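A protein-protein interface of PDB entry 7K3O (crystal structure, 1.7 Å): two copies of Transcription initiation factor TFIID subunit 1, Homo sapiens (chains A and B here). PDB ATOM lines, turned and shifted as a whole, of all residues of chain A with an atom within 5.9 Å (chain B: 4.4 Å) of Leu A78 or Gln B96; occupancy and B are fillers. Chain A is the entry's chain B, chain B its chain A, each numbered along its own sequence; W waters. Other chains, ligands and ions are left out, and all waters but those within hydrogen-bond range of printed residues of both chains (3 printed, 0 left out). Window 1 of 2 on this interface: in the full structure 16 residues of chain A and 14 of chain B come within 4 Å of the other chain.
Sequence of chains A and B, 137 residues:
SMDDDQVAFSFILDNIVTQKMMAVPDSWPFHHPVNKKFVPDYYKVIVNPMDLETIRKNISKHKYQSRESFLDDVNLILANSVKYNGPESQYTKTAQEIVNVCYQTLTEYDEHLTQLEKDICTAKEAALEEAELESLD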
ATOM      1  N   ASP A  72      -1.240 -29.073  27.680  1.00  0.00           N
ATOM      2  CA  ASP A  72      -0.884 -27.768  27.128  1.00  0.00           C
ATOM      3  C   ASP A  72      -0.275 -27.912  25.736  1.00  0.00           C
ATOM      4  O   ASP A  72      -0.576 -27.114  24.839  1.00  0.00           O
ATOM      5  CB  ASP A  72       0.086 -27.028  28.053  1.00  0.00           C
ATOM      6  CG  ASP A  72      -0.602 -26.358  29.227  1.00  0.00           C
ATOM      7  OD1 ASP A  72      -1.850 -26.236  29.240  1.00  0.00           O
ATOM      8  OD2 ASP A  72       0.132 -25.949  30.147  1.00  0.00           O
ATOM      9  N   ASP A  73       0.600 -28.912  25.541  1.00  0.00           N
ATOM     10  CA  ASP A  73       1.217 -29.108  24.226  1.00  0.00           C
ATOM     11  C   ASP A  73       0.209 -29.640  23.219  1.00  0.00           C
ATOM     12  O   ASP A  73       0.221 -29.239  22.048  1.00  0.00           O
ATOM     13  CB  ASP A  73       2.419 -30.049  24.322  1.00  0.00           C
ATOM     14  CG  ASP A  73       3.666 -29.348  24.821  1.00  0.00           C
ATOM     15  OD1 ASP A  73       3.703 -28.097  24.803  1.00  0.00           O
ATOM     16  OD2 ASP A  73       4.601 -30.042  25.245  1.00  0.00           O
ATOM     17  N   VAL A  74      -0.681 -30.534  23.651  1.00  0.00           N
ATOM     18  CA  VAL A  74      -1.732 -31.019  22.757  1.00  0.00           C
ATOM     19  C   VAL A  74      -2.619 -29.858  22.310  1.00  0.00           C
ATOM     20  O   VAL A  74      -2.936 -29.707  21.122  1.00  0.00           O
ATOM     21  CB  VAL A  74      -2.551 -32.126  23.447  1.00  0.00           C
ATOM     22  CG1 VAL A  74      -3.762 -32.491  22.590  1.00  0.00           C
ATOM     23  CG2 VAL A  74      -1.665 -33.367  23.691  1.00  0.00           C
ATOM     24  N   ASN A  75      -3.021 -29.017  23.258  1.00  0.00           N
ATOM     25  CA  ASN A  75      -3.862 -27.869  22.933  1.00  0.00           C
ATOM     26  C   ASN A  75      -3.169 -26.921  21.961  1.00  0.00           C
ATOM     27  O   ASN A  75      -3.832 -26.267  21.141  1.00  0.00           O
ATOM     28  CB  ASN A  75      -4.215 -27.119  24.220  1.00  0.00           C
ATOM     29  CG  ASN A  75      -5.423 -27.698  24.915  1.00  0.00           C
ATOM     30  OD1 ASN A  75      -6.306 -28.244  24.264  1.00  0.00           O
ATOM     31  ND2 ASN A  75      -5.483 -27.558  26.238  1.00  0.00           N
ATOM     32  N   LEU A  76      -1.844 -26.831  22.034  1.00  0.00           N
ATOM     33  CA  LEU A  76      -1.116 -25.917  21.159  1.00  0.00           C
ATOM     34  C   LEU A  76      -1.213 -26.352  19.700  1.00  0.00           C
ATOM     35  O   LEU A  76      -1.215 -25.505  18.799  1.00  0.00           O
ATOM     36  CB  LEU A  76       0.346 -25.824  21.598  1.00  0.00           C
ATOM     37  CG  LEU A  76       1.266 -24.937  20.750  1.00  0.00           C
ATOM     38  CD1 LEU A  76       0.755 -23.495  20.710  1.00  0.00           C
ATOM     39  CD2 LEU A  76       2.684 -24.994  21.304  1.00  0.00           C
ATOM     40  N   ILE A  77      -1.306 -27.657  19.453  1.00  0.00           N
ATOM     41  CA  ILE A  77      -1.529 -28.146  18.088  1.00  0.00           C
ATOM     42  C   ILE A  77      -2.790 -27.516  17.505  1.00  0.00           C
ATOM     43  O   ILE A  77      -2.798 -27.031  16.365  1.00  0.00           O
ATOM     44  CB  ILE A  77      -1.618 -29.680  18.084  1.00  0.00           C
ATOM     45  CG1 ILE A  77      -0.288 -30.277  18.543  1.00  0.00           C
ATOM     46  CG2 ILE A  77      -1.952 -30.213  16.671  1.00  0.00           C
ATOM     47  CD1 ILE A  77      -0.278 -31.821  18.574  1.00  0.00           C
ATOM     48  N   LEU A  78      -3.883 -27.546  18.266  1.00  0.00           N
ATOM     49  CA  LEU A  78      -5.131 -26.946  17.795  1.00  0.00           C
ATOM     50  C   LEU A  78      -5.007 -25.435  17.639  1.00  0.00           C
ATOM     51  O   LEU A  78      -5.470 -24.855  16.642  1.00  0.00           O
ATOM     52  CB  LEU A  78      -6.268 -27.273  18.757  1.00  0.00           C
ATOM     53  CG  LEU A  78      -7.507 -26.458  18.350  1.00  0.00           C
ATOM     54  CD1 LEU A  78      -8.145 -26.984  17.045  1.00  0.00           C
ATOM     55  CD2 LEU A  78      -8.518 -26.368  19.443  1.00  0.00           C
ATOM     56  N   ALA A  79      -4.437 -24.769  18.643  1.00  0.00           N
ATOM     57  CA  ALA A  79      -4.368 -23.313  18.591  1.00  0.00           C
ATOM     58  C   ALA A  79      -3.553 -22.862  17.391  1.00  0.00           C
ATOM     59  O   ALA A  79      -3.920 -21.895  16.706  1.00  0.00           O
ATOM     60  CB  ALA A  79      -3.785 -22.755  19.892  1.00  0.00           C
ATOM     61  N   ASN A  80      -2.457 -23.567  17.099  1.00  0.00           N
ATOM     62  CA  ASN A  80      -1.665 -23.221  15.926  1.00  0.00           C
ATOM     63  C   ASN A  80      -2.466 -23.428  14.646  1.00  0.00           C
ATOM     64  O   ASN A  80      -2.330 -22.654  13.693  1.00  0.00           O
ATOM     65  CB  ASN A  80      -0.376 -24.054  15.884  1.00  0.00           C
ATOM     66  CG  ASN A  80       0.688 -23.540  16.842  1.00  0.00           C
ATOM     67  OD1 ASN A  80       0.653 -22.386  17.286  1.00  0.00           O
ATOM     68  ND2 ASN A  80       1.655 -24.393  17.154  1.00  0.00           N
ATOM     69  N   SER A  81      -3.294 -24.476  14.597  1.00  0.00           N
ATOM     70  CA  SER A  81      -4.091 -24.713  13.396  1.00  0.00           C
ATOM     71  C   SER A  81      -5.150 -23.621  13.231  1.00  0.00           C
ATOM     72  O   SER A  81      -5.434 -23.186  12.107  1.00  0.00           O
ATOM     73  CB  SER A  81      -4.733 -26.101  13.456  1.00  0.00           C
ATOM     74  OG  SER A  81      -5.543 -26.374  12.310  1.00  0.00           O
ATOM     75  N   VAL A  82      -5.745 -23.153  14.337  1.00  0.00           N
ATOM     76  CA  VAL A  82      -6.673 -22.022  14.237  1.00  0.00           C
ATOM     77  C   VAL A  82      -5.974 -20.838  13.597  1.00  0.00           C
ATOM     78  O   VAL A  82      -6.532 -20.159  12.721  1.00  0.00           O
ATOM     79  CB  VAL A  82      -7.236 -21.647  15.629  1.00  0.00           C
ATOM     80  CG1 VAL A  82      -7.985 -20.303  15.562  1.00  0.00           C
ATOM     81  CG2 VAL A  82      -8.140 -22.755  16.138  1.00  0.00           C
ATOM     82  N   LYS A  83      -4.735 -20.569  14.017  1.00  0.00           N
ATOM     83  CA  LYS A  83      -4.015 -19.420  13.489  1.00  0.00           C
ATOM     84  C   LYS A  83      -3.580 -19.638  12.041  1.00  0.00           C
ATOM     85  O   LYS A  83      -3.769 -18.753  11.197  1.00  0.00           O
ATOM     86  CB  LYS A  83      -2.802 -19.114  14.373  1.00  0.00           C
ATOM     87  CG  LYS A  83      -1.928 -17.990  13.830  1.00  0.00           C
ATOM     88  CD  LYS A  83      -0.782 -17.646  14.772  1.00  0.00           C
ATOM     89  CE  LYS A  83       0.060 -16.531  14.190  1.00  0.00           C
ATOM     90  NZ  LYS A  83       1.239 -16.178  15.033  1.00  0.00           N
ATOM     91  N   THR A  92      -8.396 -27.749  11.167  1.00  0.00           N
ATOM     92  CA  THR A  92      -8.664 -27.343  12.539  1.00  0.00           C
ATOM     93  C   THR A  92      -9.708 -28.242  13.184  1.00  0.00           C
ATOM     94  O   THR A  92      -9.591 -28.586  14.365  1.00  0.00           O
ATOM     95  CB  THR A  92      -9.103 -25.888  12.534  1.00  0.00           C
ATOM     96  OG1 THR A  92      -8.012 -25.092  12.049  1.00  0.00           O
ATOM     97  CG2 THR A  92      -9.524 -25.404  13.938  1.00  0.00           C
ATOM     98  N   LYS A  93     -10.734 -28.632  12.423  1.00  0.00           N
ATOM     99  CA  LYS A  93     -11.714 -29.576  12.951  1.00  0.00           C
ATOM    100  C   LYS A  93     -11.056 -30.892  13.321  1.00  0.00           C
ATOM    101  O   LYS A  93     -11.351 -31.468  14.378  1.00  0.00           O
ATOM    102  CB  LYS A  93     -12.829 -29.802  11.935  1.00  0.00           C
ATOM    103  CG  LYS A  93     -13.508 -28.509  11.512  1.00  0.00           C
ATOM    104  CD  LYS A  93     -14.968 -28.719  11.161  1.00  0.00           C
ATOM    105  CE  LYS A  93     -15.652 -27.386  10.906  1.00  0.00           C
ATOM    106  NZ  LYS A  93     -16.518 -27.009  12.055  1.00  0.00           N
ATOM    107  N   ALA A  95      -7.863 -31.257  14.119  1.00  0.00           N
ATOM    108  CA  ALA A  95      -7.075 -30.974  15.318  1.00  0.00           C
ATOM    109  C   ALA A  95      -7.945 -30.954  16.571  1.00  0.00           C
ATOM    110  O   ALA A  95      -7.524 -31.437  17.629  1.00  0.00           O
ATOM    111  CB  ALA A  95      -6.345 -29.644  15.172  1.00  0.00           C
ATOM    112  N   GLN A  96      -9.157 -30.399  16.484  1.00  0.00           N
ATOM    113  CA  GLN A  96     -10.008 -30.385  17.675  1.00  0.00           C
ATOM    114  C   GLN A  96     -10.462 -31.789  18.048  1.00  0.00           C
ATOM    115  O   GLN A  96     -10.621 -32.093  19.237  1.00  0.00           O
ATOM    116  CB  GLN A  96     -11.211 -29.463  17.491  1.00  0.00           C
ATOM    117  CG  GLN A  96     -12.147 -29.413  18.747  1.00  0.00           C
ATOM    118  CD  GLN A  96     -11.566 -28.665  19.938  1.00  0.00           C
ATOM    119  OE1 GLN A  96     -11.246 -27.494  19.824  1.00  0.00           O
ATOM    120  NE2 GLN A  96     -11.511 -29.314  21.111  1.00  0.00           N
ATOM    121  N   VAL A  99      -7.670 -33.147  20.034  1.00  0.00           N
ATOM    122  CA  VAL A  99      -7.743 -32.600  21.385  1.00  0.00           C
ATOM    123  C   VAL A  99      -8.859 -33.275  22.168  1.00  0.00           C
ATOM    124  O   VAL A  99      -8.678 -33.650  23.332  1.00  0.00           O
ATOM    125  CB  VAL A  99      -7.943 -31.070  21.338  1.00  0.00           C
ATOM    126  CG1 VAL A  99      -8.283 -30.523  22.745  1.00  0.00           C
ATOM    127  CG2 VAL A  99      -6.709 -30.395  20.802  1.00  0.00           C
ATOM    128  N   LEU B  78     -12.874 -19.066  21.193  1.00  0.00           N
ATOM    129  CA  LEU B  78     -11.486 -19.516  21.088  1.00  0.00           C
ATOM    130  C   LEU B  78     -10.780 -18.865  19.904  1.00  0.00           C
ATOM    131  O   LEU B  78      -9.639 -18.398  20.033  1.00  0.00           O
ATOM    132  CB  LEU B  78     -11.453 -21.045  20.992  1.00  0.00           C
ATOM    133  CG  LEU B  78     -10.084 -21.676  20.728  1.00  0.00           C
ATOM    134  CD1 LEU B  78      -9.076 -21.177  21.780  1.00  0.00           C
ATOM    135  CD2 LEU B  78     -10.184 -23.205  20.715  1.00  0.00           C
ATOM    136  N   THR B  92      -5.716 -17.824  26.004  1.00  0.00           N
ATOM    137  CA  THR B  92      -6.111 -18.836  25.037  1.00  0.00           C
ATOM    138  C   THR B  92      -6.173 -20.197  25.703  1.00  0.00           C
ATOM    139  O   THR B  92      -7.080 -20.989  25.422  1.00  0.00           O
ATOM    140  CB  THR B  92      -5.147 -18.816  23.856  1.00  0.00           C
ATOM    141  OG1 THR B  92      -5.281 -17.554  23.188  1.00  0.00           O
ATOM    142  CG2 THR B  92      -5.454 -19.970  22.845  1.00  0.00           C
ATOM    143  N   LYS B  93      -5.261 -20.474  26.623  1.00  0.00           N
ATOM    144  CA  LYS B  93      -5.324 -21.762  27.351  1.00  0.00           C
ATOM    145  C   LYS B  93      -6.634 -21.837  28.139  1.00  0.00           C
ATOM    146  O   LYS B  93      -7.256 -22.888  28.135  1.00  0.00           O
ATOM    147  CB  LYS B  93      -4.095 -21.963  28.233  1.00  0.00           C
ATOM    148  CG  LYS B  93      -2.802 -22.162  27.459  1.00  0.00           C
ATOM    149  CD  LYS B  93      -1.633 -22.509  28.340  1.00  0.00           C
ATOM    150  CE  LYS B  93      -0.701 -21.341  28.569  1.00  0.00           C
ATOM    151  NZ  LYS B  93       0.310 -21.646  29.606  1.00  0.00           N
ATOM    152  N   THR B  94      -7.019 -20.732  28.770  1.00  0.00           N
ATOM    153  CA  THR B  94      -8.300 -20.721  29.476  1.00  0.00           C
ATOM    154  C   THR B  94      -9.463 -20.940  28.504  1.00  0.00           C
ATOM    155  O   THR B  94     -10.387 -21.723  28.785  1.00  0.00           O
ATOM    156  CB  THR B  94      -8.446 -19.407  30.249  1.00  0.00           C
ATOM    157  OG1 THR B  94      -7.421 -19.340  31.261  1.00  0.00           O
ATOM    158  CG2 THR B  94      -9.811 -19.339  30.965  1.00  0.00           C
ATOM    159  N   ALA B  95      -9.437 -20.265  27.349  1.00  0.00           N
ATOM    160  CA  ALA B  95     -10.492 -20.471  26.354  1.00  0.00           C
ATOM    161  C   ALA B  95     -10.536 -21.921  25.891  1.00  0.00           C
ATOM    162  O   ALA B  95     -11.615 -22.471  25.632  1.00  0.00           O
ATOM    163  CB  ALA B  95     -10.280 -19.549  25.146  1.00  0.00           C
ATOM    164  N   GLN B  96      -9.373 -22.545  25.742  1.00  0.00           N
ATOM    165  CA  GLN B  96      -9.359 -23.934  25.296  1.00  0.00           C
ATOM    166  C   GLN B  96      -9.931 -24.865  26.346  1.00  0.00           C
ATOM    167  O   GLN B  96     -10.609 -25.836  25.990  1.00  0.00           O
ATOM    168  CB  GLN B  96      -7.947 -24.347  24.902  1.00  0.00           C
ATOM    169  CG  GLN B  96      -7.543 -23.705  23.575  1.00  0.00           C
ATOM    170  CD  GLN B  96      -6.243 -24.242  23.039  1.00  0.00           C
ATOM    171  OE1 GLN B  96      -5.178 -23.751  23.395  1.00  0.00           O
ATOM    172  NE2 GLN B  96      -6.323 -25.262  22.179  1.00  0.00           N
ATOM    173  N   GLU B  97      -9.714 -24.579  27.633  1.00  0.00           N
ATOM    174  CA  GLU B  97     -10.355 -25.394  28.659  1.00  0.00           C
ATOM    175  C   GLU B  97     -11.873 -25.237  28.600  1.00  0.00           C
ATOM    176  O   GLU B  97     -12.608 -26.217  28.765  1.00  0.00           O
ATOM    177  CB  GLU B  97      -9.816 -25.025  30.040  1.00  0.00           C
ATOM    178  CG  GLU B  97     -10.439 -25.842  31.179  1.00  0.00           C
ATOM    179  CD  GLU B  97     -10.093 -27.329  31.136  1.00  0.00           C
ATOM    180  OE1 GLU B  97      -9.060 -27.705  30.525  1.00  0.00           O
ATOM    181  OE2 GLU B  97     -10.855 -28.124  31.738  1.00  0.00           O
ATOM    182  N   ILE B  98     -12.352 -24.016  28.331  1.00  0.00           N
ATOM    183  CA  ILE B  98     -13.788 -23.776  28.164  1.00  0.00           C
ATOM    184  C   ILE B  98     -14.339 -24.595  26.997  1.00  0.00           C
ATOM    185  O   ILE B  98     -15.370 -25.274  27.116  1.00  0.00           O
ATOM    186  CB  ILE B  98     -14.042 -22.270  27.955  1.00  0.00           C
ATOM    187  CG1 ILE B  98     -13.713 -21.476  29.238  1.00  0.00           C
ATOM    188  CG2 ILE B  98     -15.485 -22.030  27.523  1.00  0.00           C
ATOM    189  CD1 ILE B  98     -13.752 -19.936  29.061  1.00  0.00           C
ATOM    190  N   VAL B  99     -13.677 -24.520  25.841  1.00  0.00           N
ATOM    191  CA  VAL B  99     -14.116 -25.282  24.672  1.00  0.00           C
ATOM    192  C   VAL B  99     -14.025 -26.776  24.948  1.00  0.00           C
ATOM    193  O   VAL B  99     -14.941 -27.541  24.624  1.00  0.00           O
ATOM    194  CB  VAL B  99     -13.291 -24.871  23.433  1.00  0.00           C
ATOM    195  CG1 VAL B  99     -13.527 -25.840  22.248  1.00  0.00           C
ATOM    196  CG2 VAL B  99     -13.643 -23.426  23.024  1.00  0.00           C
ATOM    197  N   ASN B 100     -12.920 -27.218  25.553  1.00  0.00           N
ATOM    198  CA  ASN B 100     -12.718 -28.656  25.731  1.00  0.00           C
ATOM    199  C   ASN B 100     -13.745 -29.240  26.689  1.00  0.00           C
ATOM    200  O   ASN B 100     -14.268 -30.334  26.449  1.00  0.00           O
ATOM    201  CB  ASN B 100     -11.306 -28.941  26.231  1.00  0.00           C
ATOM    202  CG  ASN B 100     -10.243 -28.682  25.162  1.00  0.00           C
ATOM    203  OD1 ASN B 100     -10.553 -28.489  23.977  1.00  0.00           O
ATOM    204  ND2 ASN B 100      -8.992 -28.641  25.587  1.00  0.00           N
HETATM  205  O   HOH W   1      -7.759 -27.711  28.234  1.00  0.00           O
HETATM  206  O   HOH W   2      -6.204 -25.327  28.481  1.00  0.00           O
HETATM  207  O   HOH W   3      -9.331 -26.538  22.375  1.00  0.00           O
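Among the printed residues, merely in contact across the chains: Val A99 with Asn B100 (3.3 Å), Leu A78 with Gln B96 (3.7 Å), Gln A96 with Val B99 (3.7 Å), Leu A78 with Leu B78 (3.8 Å), Asp A72 with Lys B93 (3.8 Å) and Ala A79 with Gln B96 (3.9 Å).
Of the printed residues of chain B, Leu A78 touches Leu B78 (3.8 Å) and Gln B96 (3.7 Å).
Printed residues of chain A within 4 Å of Gln B96: Asn A75, Leu A78 and Ala A79.
Printed residues of chain B within 4 Å of Ala A79: Gln B96 (3.9 Å).
Printed residues of chain A within 4 Å of Leu B78: Leu A78.
Printed residues of chain A within 4 Å of Lys B93: Asp A72 (3.8 Å).
Of the printed residues of chain B, Asp A72 touches Lys B93 (3.8 Å).
Of the printed residues of chain B, Gln A96 touches Val B99 and Asn B100.
Ile B98 touches none of the printed residues of chain A.
Ala B95 touches none of the printed residues of chain A.
The nearest printed residue of chain B that does not touch Leu A78 is Asn B100 (5.4 Å).
The nearest printed residue of chain B that does not touch Val A99 is Gln B96 (5.3 Å).
Water W1 lies within hydrogen-bond range of OE1 of Glu B97 (2.6 Å), ND2 of Asn A75 (3.0 Å) and ND2 of Asn B100 (3.1 Å).
Water W2 lies within hydrogen-bond range of the backbone carbonyl oxygen (O) of Lys B93 and the side-chain amide nitrogen (ND2) of Asn A75.
Water W3 lies within hydrogen-bond range of the side-chain amide oxygen (OD1) of Asn B100, the side-chain amide nitrogen (NE2) of Gln B96 and the side-chain amide oxygen (OE1) of Gln A96.
The backbone carbonyl oxygen (O) of Gln B96 sits close to the side-chain amide nitrogen (ND2) of Asn B100.
Of the 10 printed residues of chain B, 5 touch a printed residue of chain A.
Of the 17 printed residues of chain A, 6 touch a printed residue of chain B.
Printed residues of chain A that touch a printed residue of chain B: Asp A72, Asn A75, Leu A78, Ala A79, Gln A96 and Val A99.
Hydrophobic or aromatic side chains of chain A that line the printed part of chain B: Leu A78, Ala A79 and Val A99.
Among the printed residues, 9 pairs touch across the chains.
Among the printed residues, no Asp or Glu carboxylate lies within 4 Å of a Lys or Arg side-chain nitrogen of the other chain.
Leu A78 touches its own counterpart, Leu B78.
Leu A78 touches Gln B96, but with the chains exchanged Gln A96 does not touch Leu B78 (4.5 Å).
Gln A96 touches Val B99, but with the chains exchanged Val A99 does not touch Gln B96 (5.3 Å).
6 positions are printed for both chains.
Of the 9 pairs that touch across the chains among the printed residues, 1 has its exchanged pair printed and touching as well.
The backbone carbonyl oxygen of Asn A75 is in hydrogen-bond range of the side-chain amide nitrogen of Gln B96, at 2.9 Å.
The side-chain amide nitrogen (ND2) of Asn B100 lies within hydrogen-bond range of the side-chain amide oxygen (OD1) of Asn A75 (3.0 Å).
The side-chain amide oxygen of Asn B100 sits at hydrogen-bond distance from the side-chain amide nitrogen of Gln A96, 3.1 Å away.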
